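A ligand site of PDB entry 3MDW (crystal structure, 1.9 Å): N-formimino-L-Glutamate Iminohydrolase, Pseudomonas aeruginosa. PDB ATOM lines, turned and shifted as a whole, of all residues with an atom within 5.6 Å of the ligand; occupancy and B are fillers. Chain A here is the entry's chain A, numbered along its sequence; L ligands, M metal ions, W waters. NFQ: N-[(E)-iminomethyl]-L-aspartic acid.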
ATOM      1  N   HIS A  58      17.519  34.921 -32.113  1.00  0.00           N
ATOM      2  CA  HIS A  58      16.240  34.629 -32.789  1.00  0.00           C
ATOM      3  C   HIS A  58      15.523  35.955 -33.046  1.00  0.00           C
ATOM      4  O   HIS A  58      14.828  36.472 -32.158  1.00  0.00           O
ATOM      5  CB  HIS A  58      15.329  33.738 -31.927  1.00  0.00           C
ATOM      6  CG  HIS A  58      16.017  32.533 -31.366  1.00  0.00           C
ATOM      7  ND1 HIS A  58      16.564  31.544 -32.157  1.00  0.00           N
ATOM      8  CD2 HIS A  58      16.229  32.155 -30.081  1.00  0.00           C
ATOM      9  CE1 HIS A  58      17.100  30.609 -31.386  1.00  0.00           C
ATOM     10  NE2 HIS A  58      16.891  30.945 -30.121  1.00  0.00           N
ATOM     11  N   GLN A  61      12.014  37.513 -31.818  1.00  0.00           N
ATOM     12  CA  GLN A  61      11.748  37.639 -30.387  1.00  0.00           C
ATOM     13  C   GLN A  61      11.952  39.056 -29.843  1.00  0.00           C
ATOM     14  O   GLN A  61      11.367  39.414 -28.818  1.00  0.00           O
ATOM     15  CB  GLN A  61      12.550  36.604 -29.578  1.00  0.00           C
ATOM     16  CG  GLN A  61      12.171  35.170 -29.965  1.00  0.00           C
ATOM     17  CD  GLN A  61      12.842  34.112 -29.100  1.00  0.00           C
ATOM     18  OE1 GLN A  61      13.491  34.414 -28.105  1.00  0.00           O
ATOM     19  NE2 GLN A  61      12.662  32.856 -29.498  1.00  0.00           N
ATOM     20  N   PHE A  78      10.488  29.200 -17.903  1.00  0.00           N
ATOM     21  CA  PHE A  78      10.882  29.034 -19.292  1.00  0.00           C
ATOM     22  C   PHE A  78       9.732  28.435 -20.107  1.00  0.00           C
ATOM     23  O   PHE A  78       9.476  28.856 -21.225  1.00  0.00           O
ATOM     24  CB  PHE A  78      12.112  28.111 -19.325  1.00  0.00           C
ATOM     25  CG  PHE A  78      12.512  27.634 -20.691  1.00  0.00           C
ATOM     26  CD1 PHE A  78      13.605  28.204 -21.341  1.00  0.00           C
ATOM     27  CD2 PHE A  78      11.839  26.592 -21.309  1.00  0.00           C
ATOM     28  CE1 PHE A  78      13.990  27.749 -22.606  1.00  0.00           C
ATOM     29  CE2 PHE A  78      12.212  26.135 -22.566  1.00  0.00           C
ATOM     30  CZ  PHE A  78      13.299  26.716 -23.222  1.00  0.00           C
ATOM     31  N   TRP A  79       9.017  27.465 -19.528  1.00  0.00           N
ATOM     32  CA  TRP A  79       8.004  26.727 -20.278  1.00  0.00           C
ATOM     33  C   TRP A  79       6.715  27.524 -20.501  1.00  0.00           C
ATOM     34  O   TRP A  79       6.109  27.431 -21.569  1.00  0.00           O
ATOM     35  CB  TRP A  79       7.771  25.345 -19.658  1.00  0.00           C
ATOM     36  CG  TRP A  79       9.073  24.575 -19.590  1.00  0.00           C
ATOM     37  CD1 TRP A  79       9.909  24.451 -18.508  1.00  0.00           C
ATOM     38  CD2 TRP A  79       9.714  23.865 -20.666  1.00  0.00           C
ATOM     39  NE1 TRP A  79      11.021  23.699 -18.840  1.00  0.00           N
ATOM     40  CE2 TRP A  79      10.921  23.335 -20.166  1.00  0.00           C
ATOM     41  CE3 TRP A  79       9.374  23.629 -22.010  1.00  0.00           C
ATOM     42  CZ2 TRP A  79      11.784  22.577 -20.945  1.00  0.00           C
ATOM     43  CZ3 TRP A  79      10.241  22.876 -22.782  1.00  0.00           C
ATOM     44  CH2 TRP A  79      11.437  22.366 -22.252  1.00  0.00           C
ATOM     45  N   TRP A  81       6.806  30.777 -20.583  1.00  0.00           N
ATOM     46  CA  TRP A  81       7.290  31.808 -21.508  1.00  0.00           C
ATOM     47  C   TRP A  81       7.208  31.294 -22.940  1.00  0.00           C
ATOM     48  O   TRP A  81       6.786  32.024 -23.845  1.00  0.00           O
ATOM     49  CB  TRP A  81       8.729  32.206 -21.185  1.00  0.00           C
ATOM     50  CG  TRP A  81       9.394  33.016 -22.276  1.00  0.00           C
ATOM     51  CD1 TRP A  81       9.388  34.385 -22.416  1.00  0.00           C
ATOM     52  CD2 TRP A  81      10.167  32.510 -23.381  1.00  0.00           C
ATOM     53  NE1 TRP A  81      10.101  34.753 -23.534  1.00  0.00           N
ATOM     54  CE2 TRP A  81      10.584  33.628 -24.149  1.00  0.00           C
ATOM     55  CE3 TRP A  81      10.545  31.230 -23.783  1.00  0.00           C
ATOM     56  CZ2 TRP A  81      11.370  33.495 -25.298  1.00  0.00           C
ATOM     57  CZ3 TRP A  81      11.322  31.102 -24.945  1.00  0.00           C
ATOM     58  CH2 TRP A  81      11.731  32.224 -25.684  1.00  0.00           C
ATOM     59  N   ARG A  82       7.606  30.050 -23.158  1.00  0.00           N
ATOM     60  CA  ARG A  82       7.637  29.504 -24.519  1.00  0.00           C
ATOM     61  C   ARG A  82       6.238  29.436 -25.130  1.00  0.00           C
ATOM     62  O   ARG A  82       6.076  29.677 -26.338  1.00  0.00           O
ATOM     63  CB  ARG A  82       8.296  28.129 -24.559  1.00  0.00           C
ATOM     64  CG  ARG A  82       8.735  27.712 -25.953  1.00  0.00           C
ATOM     65  CD  ARG A  82       9.413  26.344 -25.936  1.00  0.00           C
ATOM     66  NE  ARG A  82       8.477  25.250 -25.704  1.00  0.00           N
ATOM     67  CZ  ARG A  82       8.735  23.982 -25.986  1.00  0.00           C
ATOM     68  NH1 ARG A  82       9.917  23.646 -26.498  1.00  0.00           N
ATOM     69  NH2 ARG A  82       7.829  23.039 -25.757  1.00  0.00           N
ATOM     70  N   MET A  85       5.715  32.759 -26.401  1.00  0.00           N
ATOM     71  CA  MET A  85       6.531  33.006 -27.579  1.00  0.00           C
ATOM     72  C   MET A  85       5.878  32.322 -28.808  1.00  0.00           C
ATOM     73  O   MET A  85       5.800  32.916 -29.880  1.00  0.00           O
ATOM     74  CB  MET A  85       7.979  32.532 -27.360  1.00  0.00           C
ATOM     75  CG  MET A  85       8.932  32.806 -28.530  1.00  0.00           C
ATOM     76  SD  MET A  85       9.006  31.463 -29.726  1.00  0.00           S
ATOM     77  CE  MET A  85       9.880  30.194 -28.795  1.00  0.00           C
ATOM     78  N   TYR A  86       5.352  31.113 -28.610  1.00  0.00           N
ATOM     79  CA  TYR A  86       4.682  30.374 -29.684  1.00  0.00           C
ATOM     80  C   TYR A  86       3.485  31.136 -30.247  1.00  0.00           C
ATOM     81  O   TYR A  86       3.250  31.162 -31.459  1.00  0.00           O
ATOM     82  CB  TYR A  86       4.211  29.001 -29.178  1.00  0.00           C
ATOM     83  CG  TYR A  86       5.267  27.918 -29.129  1.00  0.00           C
ATOM     84  CD1 TYR A  86       6.590  28.183 -29.478  1.00  0.00           C
ATOM     85  CD2 TYR A  86       4.941  26.632 -28.741  1.00  0.00           C
ATOM     86  CE1 TYR A  86       7.554  27.185 -29.428  1.00  0.00           C
ATOM     87  CE2 TYR A  86       5.881  25.631 -28.690  1.00  0.00           C
ATOM     88  CZ  TYR A  86       7.189  25.910 -29.030  1.00  0.00           C
ATOM     89  OH  TYR A  86       8.118  24.906 -28.971  1.00  0.00           O
ATOM     90  N   TYR A 121      14.660  29.353 -37.156  1.00  0.00           N
ATOM     91  CA  TYR A 121      13.777  28.189 -37.256  1.00  0.00           C
ATOM     92  C   TYR A 121      12.349  28.489 -37.702  1.00  0.00           C
ATOM     93  O   TYR A 121      11.520  27.590 -37.760  1.00  0.00           O
ATOM     94  CB  TYR A 121      13.736  27.408 -35.936  1.00  0.00           C
ATOM     95  CG  TYR A 121      13.400  28.265 -34.730  1.00  0.00           C
ATOM     96  CD1 TYR A 121      12.119  28.794 -34.573  1.00  0.00           C
ATOM     97  CD2 TYR A 121      14.343  28.531 -33.753  1.00  0.00           C
ATOM     98  CE1 TYR A 121      11.791  29.570 -33.484  1.00  0.00           C
ATOM     99  CE2 TYR A 121      14.024  29.301 -32.636  1.00  0.00           C
ATOM    100  CZ  TYR A 121      12.748  29.821 -32.515  1.00  0.00           C
ATOM    101  OH  TYR A 121      12.403  30.588 -31.425  1.00  0.00           O
ATOM    102  N   TYR A 159      14.258  21.232 -37.359  1.00  0.00           N
ATOM    103  CA  TYR A 159      13.325  21.099 -36.248  1.00  0.00           C
ATOM    104  C   TYR A 159      12.263  20.106 -36.728  1.00  0.00           C
ATOM    105  O   TYR A 159      11.601  20.348 -37.745  1.00  0.00           O
ATOM    106  CB  TYR A 159      12.697  22.456 -35.970  1.00  0.00           C
ATOM    107  CG  TYR A 159      12.068  22.604 -34.604  1.00  0.00           C
ATOM    108  CD1 TYR A 159      12.477  23.616 -33.731  1.00  0.00           C
ATOM    109  CD2 TYR A 159      11.047  21.740 -34.188  1.00  0.00           C
ATOM    110  CE1 TYR A 159      11.896  23.765 -32.474  1.00  0.00           C
ATOM    111  CE2 TYR A 159      10.472  21.879 -32.939  1.00  0.00           C
ATOM    112  CZ  TYR A 159      10.889  22.887 -32.081  1.00  0.00           C
ATOM    113  OH  TYR A 159      10.287  22.999 -30.852  1.00  0.00           O
ATOM    114  N   HIS A 206      17.891  22.250 -33.778  1.00  0.00           N
ATOM    115  CA  HIS A 206      17.302  23.099 -32.763  1.00  0.00           C
ATOM    116  C   HIS A 206      17.743  22.671 -31.365  1.00  0.00           C
ATOM    117  O   HIS A 206      18.137  23.502 -30.541  1.00  0.00           O
ATOM    118  CB  HIS A 206      15.779  23.127 -32.831  1.00  0.00           C
ATOM    119  CG  HIS A 206      15.162  23.903 -31.711  1.00  0.00           C
ATOM    120  ND1 HIS A 206      14.854  23.342 -30.489  1.00  0.00           N
ATOM    121  CD2 HIS A 206      14.862  25.225 -31.595  1.00  0.00           C
ATOM    122  CE1 HIS A 206      14.354  24.268 -29.696  1.00  0.00           C
ATOM    123  NE2 HIS A 206      14.349  25.420 -30.340  1.00  0.00           N
ATOM    124  N   SER A 207      17.668  21.372 -31.119  1.00  0.00           N
ATOM    125  CA  SER A 207      17.972  20.792 -29.804  1.00  0.00           C
ATOM    126  C   SER A 207      17.861  19.271 -29.925  1.00  0.00           C
ATOM    127  O   SER A 207      17.439  18.755 -30.963  1.00  0.00           O
ATOM    128  CB  SER A 207      16.956  21.293 -28.771  1.00  0.00           C
ATOM    129  OG  SER A 207      15.644  20.912 -29.157  1.00  0.00           O
ATOM    130  N   ARG A 209      15.820  17.660 -28.212  1.00  0.00           N
ATOM    131  CA  ARG A 209      14.381  17.472 -28.123  1.00  0.00           C
ATOM    132  C   ARG A 209      13.724  17.439 -29.511  1.00  0.00           C
ATOM    133  O   ARG A 209      12.796  16.661 -29.764  1.00  0.00           O
ATOM    134  CB  ARG A 209      13.741  18.585 -27.294  1.00  0.00           C
ATOM    135  CG  ARG A 209      13.970  18.458 -25.795  1.00  0.00           C
ATOM    136  CD  ARG A 209      13.644  19.747 -25.062  1.00  0.00           C
ATOM    137  NE  ARG A 209      14.664  20.784 -25.286  1.00  0.00           N
ATOM    138  CZ  ARG A 209      14.419  21.975 -25.816  1.00  0.00           C
ATOM    139  NH1 ARG A 209      13.189  22.302 -26.188  1.00  0.00           N
ATOM    140  NH2 ARG A 209      15.413  22.857 -25.967  1.00  0.00           N
ATOM    141  N   HIS A 232      20.967  24.113 -29.474  1.00  0.00           N
ATOM    142  CA  HIS A 232      20.626  24.434 -28.089  1.00  0.00           C
ATOM    143  C   HIS A 232      20.835  23.171 -27.269  1.00  0.00           C
ATOM    144  O   HIS A 232      20.392  22.108 -27.674  1.00  0.00           O
ATOM    145  CB  HIS A 232      19.150  24.767 -27.908  1.00  0.00           C
ATOM    146  CG  HIS A 232      18.711  26.070 -28.479  1.00  0.00           C
ATOM    147  ND1 HIS A 232      17.764  26.161 -29.478  1.00  0.00           N
ATOM    148  CD2 HIS A 232      19.050  27.343 -28.160  1.00  0.00           C
ATOM    149  CE1 HIS A 232      17.546  27.439 -29.758  1.00  0.00           C
ATOM    150  NE2 HIS A 232      18.313  28.172 -28.980  1.00  0.00           N
ATOM    151  N   GLU A 235      19.890  23.790 -21.593  1.00  0.00           N
ATOM    152  CA  GLU A 235      19.450  25.083 -21.074  1.00  0.00           C
ATOM    153  C   GLU A 235      18.600  24.955 -19.797  1.00  0.00           C
ATOM    154  O   GLU A 235      18.770  25.722 -18.850  1.00  0.00           O
ATOM    155  CB  GLU A 235      18.681  25.883 -22.134  1.00  0.00           C
ATOM    156  CG  GLU A 235      18.360  27.316 -21.694  1.00  0.00           C
ATOM    157  CD  GLU A 235      17.560  28.115 -22.710  1.00  0.00           C
ATOM    158  OE1 GLU A 235      17.094  27.527 -23.705  1.00  0.00           O
ATOM    159  OE2 GLU A 235      17.415  29.353 -22.514  1.00  0.00           O
ATOM    160  N   HIS A 269      23.920  27.829 -24.697  1.00  0.00           N
ATOM    161  CA  HIS A 269      23.599  27.707 -23.266  1.00  0.00           C
ATOM    162  C   HIS A 269      24.497  26.719 -22.518  1.00  0.00           C
ATOM    163  O   HIS A 269      25.319  27.126 -21.698  1.00  0.00           O
ATOM    164  CB  HIS A 269      22.113  27.382 -23.052  1.00  0.00           C
ATOM    165  CG  HIS A 269      21.193  28.302 -23.788  1.00  0.00           C
ATOM    166  ND1 HIS A 269      21.200  29.669 -23.595  1.00  0.00           N
ATOM    167  CD2 HIS A 269      20.255  28.064 -24.736  1.00  0.00           C
ATOM    168  CE1 HIS A 269      20.304  30.237 -24.381  1.00  0.00           C
ATOM    169  NE2 HIS A 269      19.713  29.282 -25.085  1.00  0.00           N
ATOM    170  N   THR A 294      19.439  36.593 -21.422  1.00  0.00           N
ATOM    171  CA  THR A 294      18.285  35.746 -21.686  1.00  0.00           C
ATOM    172  C   THR A 294      18.200  34.603 -20.668  1.00  0.00           C
ATOM    173  O   THR A 294      17.124  34.294 -20.165  1.00  0.00           O
ATOM    174  CB  THR A 294      18.290  35.205 -23.138  1.00  0.00           C
ATOM    175  OG1 THR A 294      17.954  36.271 -24.050  1.00  0.00           O
ATOM    176  CG2 THR A 294      17.259  34.067 -23.285  1.00  0.00           C
ATOM    177  N   LEU A 298      15.027  34.075 -18.375  1.00  0.00           N
ATOM    178  CA  LEU A 298      14.248  32.844 -18.426  1.00  0.00           C
ATOM    179  C   LEU A 298      14.404  31.912 -17.215  1.00  0.00           C
ATOM    180  O   LEU A 298      13.808  30.833 -17.165  1.00  0.00           O
ATOM    181  CB  LEU A 298      14.568  32.059 -19.714  1.00  0.00           C
ATOM    182  CG  LEU A 298      14.244  32.799 -21.000  1.00  0.00           C
ATOM    183  CD1 LEU A 298      14.622  31.961 -22.215  1.00  0.00           C
ATOM    184  CD2 LEU A 298      12.748  33.145 -21.030  1.00  0.00           C
ATOM    185  N   ASP A 300      17.111  30.226 -16.376  1.00  0.00           N
ATOM    186  CA  ASP A 300      17.822  29.011 -16.773  1.00  0.00           C
ATOM    187  C   ASP A 300      18.800  28.541 -15.705  1.00  0.00           C
ATOM    188  O   ASP A 300      18.889  27.342 -15.415  1.00  0.00           O
ATOM    189  CB  ASP A 300      18.578  29.225 -18.091  1.00  0.00           C
ATOM    190  CG  ASP A 300      17.653  29.323 -19.304  1.00  0.00           C
ATOM    191  OD1 ASP A 300      16.546  28.750 -19.262  1.00  0.00           O
ATOM    192  OD2 ASP A 300      18.045  29.975 -20.294  1.00  0.00           O
ATOM    193  N   ASP A 320      20.264  36.302 -28.021  1.00  0.00           N
ATOM    194  CA  ASP A 320      19.219  35.264 -27.966  1.00  0.00           C
ATOM    195  C   ASP A 320      17.767  35.762 -28.091  1.00  0.00           C
ATOM    196  O   ASP A 320      17.288  35.978 -29.204  1.00  0.00           O
ATOM    197  CB  ASP A 320      19.403  34.404 -26.704  1.00  0.00           C
ATOM    198  CG  ASP A 320      18.523  33.167 -26.715  1.00  0.00           C
ATOM    199  OD1 ASP A 320      17.865  32.895 -27.743  1.00  0.00           O
ATOM    200  OD2 ASP A 320      18.491  32.447 -25.691  1.00  0.00           O
HETATM  201  C   NFQ L   1      13.764  28.779 -28.799  1.00  0.00           C
HETATM  202  N   NFQ L   1      14.520  29.497 -26.582  1.00  0.00           N
HETATM  203  O1  NFQ L   1      13.651  29.997 -29.080  1.00  0.00           O
HETATM  204  O2  NFQ L   1      13.500  27.924 -29.666  1.00  0.00           O
HETATM  205  CA  NFQ L   1      14.222  28.318 -27.411  1.00  0.00           C
HETATM  206  CB  NFQ L   1      13.141  27.411 -26.774  1.00  0.00           C
HETATM  207  CF  NFQ L   1      15.290  29.396 -25.333  1.00  0.00           C
HETATM  208  NF  NFQ L   1      15.671  30.441 -24.755  1.00  0.00           N
HETATM  209  CG  NFQ L   1      13.465  25.912 -26.891  1.00  0.00           C
HETATM  210  OD1 NFQ L   1      14.631  25.522 -26.659  1.00  0.00           O
HETATM  211  OD2 NFQ L   1      12.531  25.129 -27.179  1.00  0.00           O
HETATM  212 ZN    ZN M   1      18.124  30.290 -28.600  1.00  0.00          ZN
HETATM  213  O   HOH W   1      17.034  25.438 -24.914  1.00  0.00           O
HETATM  214  O   HOH W   2      15.085  32.485 -26.786  1.00  0.00           O
HETATM  215  O   HOH W   3      17.813  30.164 -26.567  1.00  0.00           O
HETATM  216  O   HOH W   4      10.890  25.252 -29.448  1.00  0.00           O
HETATM  217  O   HOH W   5      11.267  27.288 -30.967  1.00  0.00           O
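OH of Tyr 121 lies within hydrogen-bond range of NE2 of Gln 61, 3.0 Å away.
O of His 206 lies within hydrogen-bond range of ND1 of His 232, at 2.9 Å.
OG of Ser 207 is in hydrogen-bond range of ND1 of His 206.
N of Arg 209 lies close to OG of Ser 207, at 3.4 Å.
The side-chain carboxylate of Glu 235 sits close to a ring nitrogen (NE2) of His 269, 3.4 Å away.
The guanidinium group of Arg 82 lies close to the side-chain hydroxyl of Tyr 86 (3.3 Å).
N of His 58 lies within hydrogen-bond range of O of Asp 320, 3.1 Å away.
A ring nitrogen (NE2) of His 269 sits close to the side-chain carboxylate (OD2) of Asp 320, 3.4 Å away.
Water W4 lies within hydrogen-bond range of OH of Tyr 159 (2.7 Å), OD2 of the ligand (2.8 Å), OH of Tyr 86 (2.8 Å) and NH1 of Arg 82 (3.5 Å).
Water W3 lies within hydrogen-bond range of OD2 of Asp 320 (2.5 Å), NE2 of His 269 (2.6 Å) and NF of the ligand (2.8 Å).
Water W2 lies within hydrogen-bond range of OE1 of Gln 61, NF of the ligand and OD1 of Asp 320.
Water W1 lies within hydrogen-bond range of the side-chain carboxylate of Glu 235, an oxygen (OD1) of the ligand and the guanidinium group of Arg 209.
Merely in contact with the ligand: His 58 (3.5 Å), Phe 78 (3.4 Å), Trp 81 (3.9 Å), Met 85 (3.8 Å) and Leu 298 (3.1 Å).
12 residues have an atom within 4 Å of the ligand: His 58, Gln 61, Phe 78, Trp 81, Arg 82, Met 85, Tyr 121, His 206, Arg 209, Glu 235, Leu 298 and Asp 320.
OH of Tyr 121 is in hydrogen-bond range of O1 of the ligand, at 2.7 Å.
An oxygen (O2) of the ligand sits at hydrogen-bond distance from a ring nitrogen (NE2) of His 206 (2.7 Å).
The guanidinium group (NH2) of Arg 209 lies within salt-bridge range of an oxygen (OD1) of the ligand (2.9 Å).
A nitrogen (NF) of the ligand lies within salt-bridge range of the side-chain carboxylate (OE2) of Glu 235, at 3.0 Å.
An oxygen (O1) of the ligand lies within hydrogen-bond range of the side-chain amide nitrogen (NE2) of Gln 61 (3.1 Å).
OD2 of the ligand lies within salt-bridge range of NH1 of Arg 82.
The side-chain carboxylate of Asp 320 is in salt-bridge range of a nitrogen (NF) of the ligand (3.6 Å).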
